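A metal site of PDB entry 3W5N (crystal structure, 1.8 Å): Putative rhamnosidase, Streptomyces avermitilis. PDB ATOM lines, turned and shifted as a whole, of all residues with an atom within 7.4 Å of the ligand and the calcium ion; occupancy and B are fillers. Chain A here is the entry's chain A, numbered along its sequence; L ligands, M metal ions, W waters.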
ATOM      1  N   PRO A 148      28.460  33.786   6.828  1.00  0.00           N
ATOM      2  CA  PRO A 148      27.686  32.954   5.890  1.00  0.00           C
ATOM      3  C   PRO A 148      27.419  31.531   6.364  1.00  0.00           C
ATOM      4  O   PRO A 148      26.402  30.945   5.972  1.00  0.00           O
ATOM      5  CB  PRO A 148      28.534  32.972   4.601  1.00  0.00           C
ATOM      6  CG  PRO A 148      29.368  34.203   4.705  1.00  0.00           C
ATOM      7  CD  PRO A 148      29.676  34.343   6.191  1.00  0.00           C
ATOM      8  N   ALA A 149      28.278  30.973   7.215  1.00  0.00           N
ATOM      9  CA  ALA A 149      28.036  29.609   7.710  1.00  0.00           C
ATOM     10  C   ALA A 149      26.782  29.559   8.612  1.00  0.00           C
ATOM     11  O   ALA A 149      26.174  28.492   8.807  1.00  0.00           O
ATOM     12  CB  ALA A 149      29.264  29.079   8.457  1.00  0.00           C
ATOM     13  N   ASN A 150      26.396  30.717   9.132  1.00  0.00           N
ATOM     14  CA  ASN A 150      25.171  30.828   9.927  1.00  0.00           C
ATOM     15  C   ASN A 150      23.997  31.309   9.077  1.00  0.00           C
ATOM     16  O   ASN A 150      22.935  30.669   9.038  1.00  0.00           O
ATOM     17  CB  ASN A 150      25.379  31.742  11.147  1.00  0.00           C
ATOM     18  CG  ASN A 150      24.132  31.863  12.003  1.00  0.00           C
ATOM     19  OD1 ASN A 150      23.398  32.851  11.923  1.00  0.00           O
ATOM     20  ND2 ASN A 150      23.848  30.816  12.796  1.00  0.00           N
ATOM     21  N   ALA A 152      23.080  33.733   5.284  1.00  0.00           N
ATOM     22  CA  ALA A 152      23.381  34.584   4.151  1.00  0.00           C
ATOM     23  C   ALA A 152      22.062  34.785   3.429  1.00  0.00           C
ATOM     24  O   ALA A 152      21.135  33.971   3.597  1.00  0.00           O
ATOM     25  CB  ALA A 152      24.409  33.906   3.242  1.00  0.00           C
ATOM     26  N   PRO A 153      21.943  35.875   2.644  1.00  0.00           N
ATOM     27  CA  PRO A 153      20.690  36.106   1.895  1.00  0.00           C
ATOM     28  C   PRO A 153      20.485  35.050   0.799  1.00  0.00           C
ATOM     29  O   PRO A 153      21.449  34.387   0.385  1.00  0.00           O
ATOM     30  CB  PRO A 153      20.909  37.491   1.264  1.00  0.00           C
ATOM     31  CG  PRO A 153      22.384  37.678   1.234  1.00  0.00           C
ATOM     32  CD  PRO A 153      22.893  36.989   2.456  1.00  0.00           C
ATOM     33  N   ALA A 178      28.412  22.947  -3.349  1.00  0.00           N
ATOM     34  CA  ALA A 178      27.908  24.257  -2.930  1.00  0.00           C
ATOM     35  C   ALA A 178      26.646  24.109  -2.118  1.00  0.00           C
ATOM     36  O   ALA A 178      25.791  23.260  -2.413  1.00  0.00           O
ATOM     37  CB  ALA A 178      27.638  25.154  -4.141  1.00  0.00           C
ATOM     38  N   ASP A 179      26.538  24.947  -1.094  1.00  0.00           N
ATOM     39  CA  ASP A 179      25.301  25.241  -0.417  1.00  0.00           C
ATOM     40  C   ASP A 179      24.828  26.592  -0.996  1.00  0.00           C
ATOM     41  O   ASP A 179      25.326  27.632  -0.577  1.00  0.00           O
ATOM     42  CB  ASP A 179      25.574  25.350   1.089  1.00  0.00           C
ATOM     43  CG  ASP A 179      24.342  25.672   1.892  1.00  0.00           C
ATOM     44  OD1 ASP A 179      23.316  26.018   1.288  1.00  0.00           O
ATOM     45  OD2 ASP A 179      24.378  25.566   3.139  1.00  0.00           O
ATOM     46  N   ASN A 180      23.888  26.612  -1.960  1.00  0.00           N
ATOM     47  CA  ASN A 180      23.125  25.444  -2.432  1.00  0.00           C
ATOM     48  C   ASN A 180      23.439  24.918  -3.831  1.00  0.00           C
ATOM     49  O   ASN A 180      23.317  23.702  -4.070  1.00  0.00           O
ATOM     50  CB  ASN A 180      21.613  25.747  -2.348  1.00  0.00           C
ATOM     51  CG  ASN A 180      21.126  25.774  -0.924  1.00  0.00           C
ATOM     52  OD1 ASN A 180      20.966  26.849  -0.320  1.00  0.00           O
ATOM     53  ND2 ASN A 180      20.937  24.589  -0.342  1.00  0.00           N
ATOM     54  N   VAL A 181      23.820  25.796  -4.755  1.00  0.00           N
ATOM     55  CA  VAL A 181      24.096  25.370  -6.141  1.00  0.00           C
ATOM     56  C   VAL A 181      25.254  26.177  -6.739  1.00  0.00           C
ATOM     57  O   VAL A 181      25.589  27.258  -6.222  1.00  0.00           O
ATOM     58  CB  VAL A 181      22.850  25.502  -7.071  1.00  0.00           C
ATOM     59  CG1 VAL A 181      21.720  24.577  -6.619  1.00  0.00           C
ATOM     60  CG2 VAL A 181      22.378  26.948  -7.182  1.00  0.00           C
ATOM     61  N   ASP A 199      17.743  20.760  -6.435  1.00  0.00           N
ATOM     62  CA  ASP A 199      18.536  20.688  -5.209  1.00  0.00           C
ATOM     63  C   ASP A 199      17.791  20.061  -4.038  1.00  0.00           C
ATOM     64  O   ASP A 199      16.758  20.575  -3.585  1.00  0.00           O
ATOM     65  CB  ASP A 199      19.076  22.059  -4.798  1.00  0.00           C
ATOM     66  CG  ASP A 199      19.918  21.996  -3.531  1.00  0.00           C
ATOM     67  OD1 ASP A 199      20.762  21.077  -3.423  1.00  0.00           O
ATOM     68  OD2 ASP A 199      19.742  22.857  -2.641  1.00  0.00           O
ATOM     69  N   ASN A 200      18.323  18.950  -3.537  1.00  0.00           N
ATOM     70  CA  ASN A 200      17.901  18.418  -2.255  1.00  0.00           C
ATOM     71  C   ASN A 200      19.104  18.177  -1.337  1.00  0.00           C
ATOM     72  O   ASN A 200      19.612  17.051  -1.264  1.00  0.00           O
ATOM     73  CB  ASN A 200      17.044  17.158  -2.417  1.00  0.00           C
ATOM     74  CG  ASN A 200      16.082  16.973  -1.260  1.00  0.00           C
ATOM     75  OD1 ASN A 200      16.491  16.775  -0.109  1.00  0.00           O
ATOM     76  ND2 ASN A 200      14.781  17.048  -1.563  1.00  0.00           N
ATOM     77  N   GLU A 201      19.554  19.235  -0.667  1.00  0.00           N
ATOM     78  CA  GLU A 201      20.779  19.214   0.149  1.00  0.00           C
ATOM     79  C   GLU A 201      21.950  18.663  -0.656  1.00  0.00           C
ATOM     80  O   GLU A 201      22.734  17.850  -0.184  1.00  0.00           O
ATOM     81  CB  GLU A 201      20.569  18.460   1.475  1.00  0.00           C
ATOM     82  CG  GLU A 201      19.368  19.001   2.251  1.00  0.00           C
ATOM     83  CD  GLU A 201      19.234  18.455   3.663  1.00  0.00           C
ATOM     84  OE1 GLU A 201      19.951  17.504   4.044  1.00  0.00           O
ATOM     85  OE2 GLU A 201      18.371  18.984   4.399  1.00  0.00           O
ATOM     86  N   GLY A 202      22.028  19.127  -1.908  1.00  0.00           N
ATOM     87  CA  GLY A 202      23.113  18.788  -2.820  1.00  0.00           C
ATOM     88  C   GLY A 202      24.510  19.080  -2.300  1.00  0.00           C
ATOM     89  O   GLY A 202      25.484  18.466  -2.755  1.00  0.00           O
ATOM     90  N   TRP A 203      24.626  19.997  -1.351  1.00  0.00           N
ATOM     91  CA  TRP A 203      25.898  20.298  -0.709  1.00  0.00           C
ATOM     92  C   TRP A 203      26.552  19.074  -0.061  1.00  0.00           C
ATOM     93  O   TRP A 203      27.764  19.022   0.074  1.00  0.00           O
ATOM     94  CB  TRP A 203      25.769  21.447   0.298  1.00  0.00           C
ATOM     95  CG  TRP A 203      24.777  21.233   1.425  1.00  0.00           C
ATOM     96  CD1 TRP A 203      23.498  21.684   1.488  1.00  0.00           C
ATOM     97  CD2 TRP A 203      25.017  20.516   2.645  1.00  0.00           C
ATOM     98  NE1 TRP A 203      22.910  21.294   2.686  1.00  0.00           N
ATOM     99  CE2 TRP A 203      23.829  20.587   3.405  1.00  0.00           C
ATOM    100  CE3 TRP A 203      26.138  19.859   3.174  1.00  0.00           C
ATOM    101  CZ2 TRP A 203      23.716  19.983   4.675  1.00  0.00           C
ATOM    102  CZ3 TRP A 203      26.019  19.255   4.436  1.00  0.00           C
ATOM    103  CH2 TRP A 203      24.833  19.327   5.160  1.00  0.00           C
ATOM    104  N   ARG A 204      25.727  18.097   0.335  1.00  0.00           N
ATOM    105  CA  ARG A 204      26.221  16.855   0.949  1.00  0.00           C
ATOM    106  C   ARG A 204      26.934  15.950  -0.018  1.00  0.00           C
ATOM    107  O   ARG A 204      27.627  15.019   0.401  1.00  0.00           O
ATOM    108  CB  ARG A 204      25.066  16.038   1.534  1.00  0.00           C
ATOM    109  CG  ARG A 204      24.290  16.732   2.630  1.00  0.00           C
ATOM    110  CD  ARG A 204      23.128  15.867   3.067  1.00  0.00           C
ATOM    111  NE  ARG A 204      22.391  16.491   4.149  1.00  0.00           N
ATOM    112  CZ  ARG A 204      22.780  16.492   5.420  1.00  0.00           C
ATOM    113  NH1 ARG A 204      23.901  15.878   5.775  1.00  0.00           N
ATOM    114  NH2 ARG A 204      22.034  17.098   6.333  1.00  0.00           N
ATOM    115  N   SER A 227      24.630  30.010  -5.692  1.00  0.00           N
ATOM    116  CA  SER A 227      23.403  30.595  -5.191  1.00  0.00           C
ATOM    117  C   SER A 227      22.939  29.894  -3.922  1.00  0.00           C
ATOM    118  O   SER A 227      23.043  28.672  -3.784  1.00  0.00           O
ATOM    119  CB  SER A 227      22.295  30.538  -6.242  1.00  0.00           C
ATOM    120  OG  SER A 227      22.706  31.169  -7.445  1.00  0.00           O
ATOM    121  N   ASN A 228      22.419  30.698  -3.002  1.00  0.00           N
ATOM    122  CA  ASN A 228      21.820  30.209  -1.765  1.00  0.00           C
ATOM    123  C   ASN A 228      20.293  30.155  -1.958  1.00  0.00           C
ATOM    124  O   ASN A 228      19.693  31.125  -2.397  1.00  0.00           O
ATOM    125  CB  ASN A 228      22.183  31.182  -0.636  1.00  0.00           C
ATOM    126  CG  ASN A 228      21.815  30.668   0.754  1.00  0.00           C
ATOM    127  OD1 ASN A 228      21.571  29.498   0.973  1.00  0.00           O
ATOM    128  ND2 ASN A 228      21.811  31.587   1.716  1.00  0.00           N
ATOM    129  N   ALA A 229      19.682  29.026  -1.611  1.00  0.00           N
ATOM    130  CA  ALA A 229      18.279  28.773  -1.987  1.00  0.00           C
ATOM    131  C   ALA A 229      17.256  29.512  -1.128  1.00  0.00           C
ATOM    132  O   ALA A 229      16.134  29.788  -1.581  1.00  0.00           O
ATOM    133  CB  ALA A 229      17.996  27.285  -1.948  1.00  0.00           C
ATOM    134  N   SER A 230      17.631  29.814   0.099  1.00  0.00           N
ATOM    135  CA  SER A 230      16.757  30.511   1.031  1.00  0.00           C
ATOM    136  C   SER A 230      17.641  31.170   2.075  1.00  0.00           C
ATOM    137  O   SER A 230      18.818  30.828   2.192  1.00  0.00           O
ATOM    138  CB  SER A 230      15.791  29.531   1.698  1.00  0.00           C
ATOM    139  OG  SER A 230      16.483  28.645   2.563  1.00  0.00           O
ATOM    140  N   VAL A 231      17.076  32.086   2.861  1.00  0.00           N
ATOM    141  CA  VAL A 231      17.826  32.676   3.973  1.00  0.00           C
ATOM    142  C   VAL A 231      18.296  31.610   4.955  1.00  0.00           C
ATOM    143  O   VAL A 231      17.505  30.821   5.486  1.00  0.00           O
ATOM    144  CB  VAL A 231      17.010  33.765   4.691  1.00  0.00           C
ATOM    145  CG1 VAL A 231      17.815  34.384   5.817  1.00  0.00           C
ATOM    146  CG2 VAL A 231      16.585  34.841   3.706  1.00  0.00           C
ATOM    147  N   GLY A 232      19.606  31.585   5.196  1.00  0.00           N
ATOM    148  CA  GLY A 232      20.283  30.540   5.938  1.00  0.00           C
ATOM    149  C   GLY A 232      21.698  30.344   5.401  1.00  0.00           C
ATOM    150  O   GLY A 232      22.182  31.179   4.612  1.00  0.00           O
ATOM    151  N   PRO A 233      22.381  29.272   5.824  1.00  0.00           N
ATOM    152  CA  PRO A 233      23.813  29.113   5.510  1.00  0.00           C
ATOM    153  C   PRO A 233      24.106  29.059   4.016  1.00  0.00           C
ATOM    154  O   PRO A 233      23.280  28.575   3.243  1.00  0.00           O
ATOM    155  CB  PRO A 233      24.196  27.792   6.191  1.00  0.00           C
ATOM    156  CG  PRO A 233      23.118  27.529   7.194  1.00  0.00           C
ATOM    157  CD  PRO A 233      21.870  28.157   6.647  1.00  0.00           C
ATOM    158  N   ALA A 234      25.268  29.563   3.619  1.00  0.00           N
ATOM    159  CA  ALA A 234      25.709  29.506   2.235  1.00  0.00           C
ATOM    160  C   ALA A 234      27.217  29.352   2.202  1.00  0.00           C
ATOM    161  O   ALA A 234      27.933  29.815   3.122  1.00  0.00           O
ATOM    162  CB  ALA A 234      25.302  30.758   1.474  1.00  0.00           C
ATOM    163  N   GLY A 235      27.704  28.751   1.130  1.00  0.00           N
ATOM    164  CA  GLY A 235      29.134  28.580   0.969  1.00  0.00           C
ATOM    165  C   GLY A 235      29.402  27.560  -0.118  1.00  0.00           C
ATOM    166  O   GLY A 235      28.562  26.711  -0.388  1.00  0.00           O
ATOM    167  N   PRO A 291      27.965  24.269   9.397  1.00  0.00           N
ATOM    168  CA  PRO A 291      26.908  23.257   9.523  1.00  0.00           C
ATOM    169  C   PRO A 291      27.130  21.984   8.691  1.00  0.00           C
ATOM    170  O   PRO A 291      26.367  21.019   8.841  1.00  0.00           O
ATOM    171  CB  PRO A 291      25.670  23.994   9.031  1.00  0.00           C
ATOM    172  CG  PRO A 291      26.180  25.041   8.090  1.00  0.00           C
ATOM    173  CD  PRO A 291      27.522  25.452   8.634  1.00  0.00           C
ATOM    174  N   TRP A 292      28.160  21.985   7.841  1.00  0.00           N
ATOM    175  CA  TRP A 292      28.238  21.008   6.751  1.00  0.00           C
ATOM    176  C   TRP A 292      28.950  19.687   7.105  1.00  0.00           C
ATOM    177  O   TRP A 292      28.751  18.677   6.426  1.00  0.00           O
ATOM    178  CB  TRP A 292      28.862  21.647   5.513  1.00  0.00           C
ATOM    179  CG  TRP A 292      28.163  22.928   5.103  1.00  0.00           C
ATOM    180  CD1 TRP A 292      26.911  23.056   4.550  1.00  0.00           C
ATOM    181  CD2 TRP A 292      28.688  24.263   5.196  1.00  0.00           C
ATOM    182  NE1 TRP A 292      26.621  24.392   4.316  1.00  0.00           N
ATOM    183  CE2 TRP A 292      27.705  25.148   4.682  1.00  0.00           C
ATOM    184  CE3 TRP A 292      29.904  24.806   5.666  1.00  0.00           C
ATOM    185  CZ2 TRP A 292      27.879  26.537   4.637  1.00  0.00           C
ATOM    186  CZ3 TRP A 292      30.086  26.195   5.616  1.00  0.00           C
ATOM    187  CH2 TRP A 292      29.080  27.040   5.103  1.00  0.00           C
HETATM  188  C1  LIG L   1      19.683  22.532   4.456  1.00  0.00           C
HETATM  189  C2  LIG L   1      19.558  23.329   3.157  1.00  0.00           C
HETATM  190  C3  LIG L   1      20.126  24.752   3.342  1.00  0.00           C
HETATM  191  C4  LIG L   1      21.565  24.713   3.855  1.00  0.00           C
HETATM  192  C5  LIG L   1      21.636  23.916   5.163  1.00  0.00           C
HETATM  193  C6  LIG L   1      23.066  23.698   5.642  1.00  0.00           C
HETATM  194  O1  LIG L   1      18.756  23.049   5.417  1.00  0.00           O
HETATM  195  O2  LIG L   1      20.274  22.615   2.155  1.00  0.00           O
HETATM  196  O3  LIG L   1      20.088  25.587   2.167  1.00  0.00           O
HETATM  197  O4  LIG L   1      21.965  26.098   3.954  1.00  0.00           O
HETATM  198  O5  LIG L   1      21.017  22.614   5.010  1.00  0.00           O
HETATM  199 CA    CA M   1      21.589  27.395   2.021  1.00  0.00          CA
HETATM  200  O   HOH W   1      16.171  24.766   4.291  1.00  0.00           O
HETATM  201  O   HOH W   2      19.801  28.456   3.275  1.00  0.00           O
HETATM  202  O   HOH W   3      18.816  21.793   0.077  1.00  0.00           O
HETATM  203  O   HOH W   4      17.518  26.125   1.711  1.00  0.00           O
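CG of Glu 201 touches O2 of the ligand (3.7 Å). Trp 292 touches the ligand.
The backbone carbonyl oxygen of Gly 235 sits at hydrogen-bond distance from the backbone NH of Asp 179 (2.8 Å). O of Ser 230 sits at hydrogen-bond distance from ND2 of Asn 228, at 3.1 Å. The backbone carbonyl oxygen of Gly 232 lies within hydrogen-bond range of the side-chain amide nitrogen of Asn 228 (2.9 Å). The side-chain amide nitrogen of Asn 228 is in hydrogen-bond range of the backbone carbonyl oxygen of Ala 152, 3.1 Å away. The side-chain amide nitrogen (ND2) of Asn 228 sits at hydrogen-bond distance from the backbone carbonyl oxygen (O) of Pro 153, 3.1 Å away. OD1 of Asn 180 lies close to N of Ala 229. ND2 of Asn 180 lies within hydrogen-bond range of OD2 of Asp 199, 3.1 Å away. The side-chain carboxylate (OE1) of Glu 201 is in salt-bridge range of the guanidinium group (NE) of Arg 204 (2.6 Å).
The calcium ion is bound by OD1 of Asp 179, OD1 of Asn 228, O3 of the ligand, O4 of the ligand, O of Pro 233, water W2 and OD1 of Asn 180. The calcium ion has seven donor atoms within binding distance.
Within 4 Å of the calcium ion: Asp 179, Asn 180, Asn 228 and Pro 233. The nearest printed residue that does not touch the calcium ion is Ala 229 (4.4 Å).
An oxygen (O2) of the ligand is in hydrogen-bond range of the indole nitrogen of Trp 203, 3.0 Å away.
Water W3 lies within hydrogen-bond range of an oxygen (O2) of the ligand (2.7 Å), the backbone NH (N) of Glu 201 (2.8 Å) and the side-chain carboxylate (OD2) of Asp 199 (3.1 Å).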
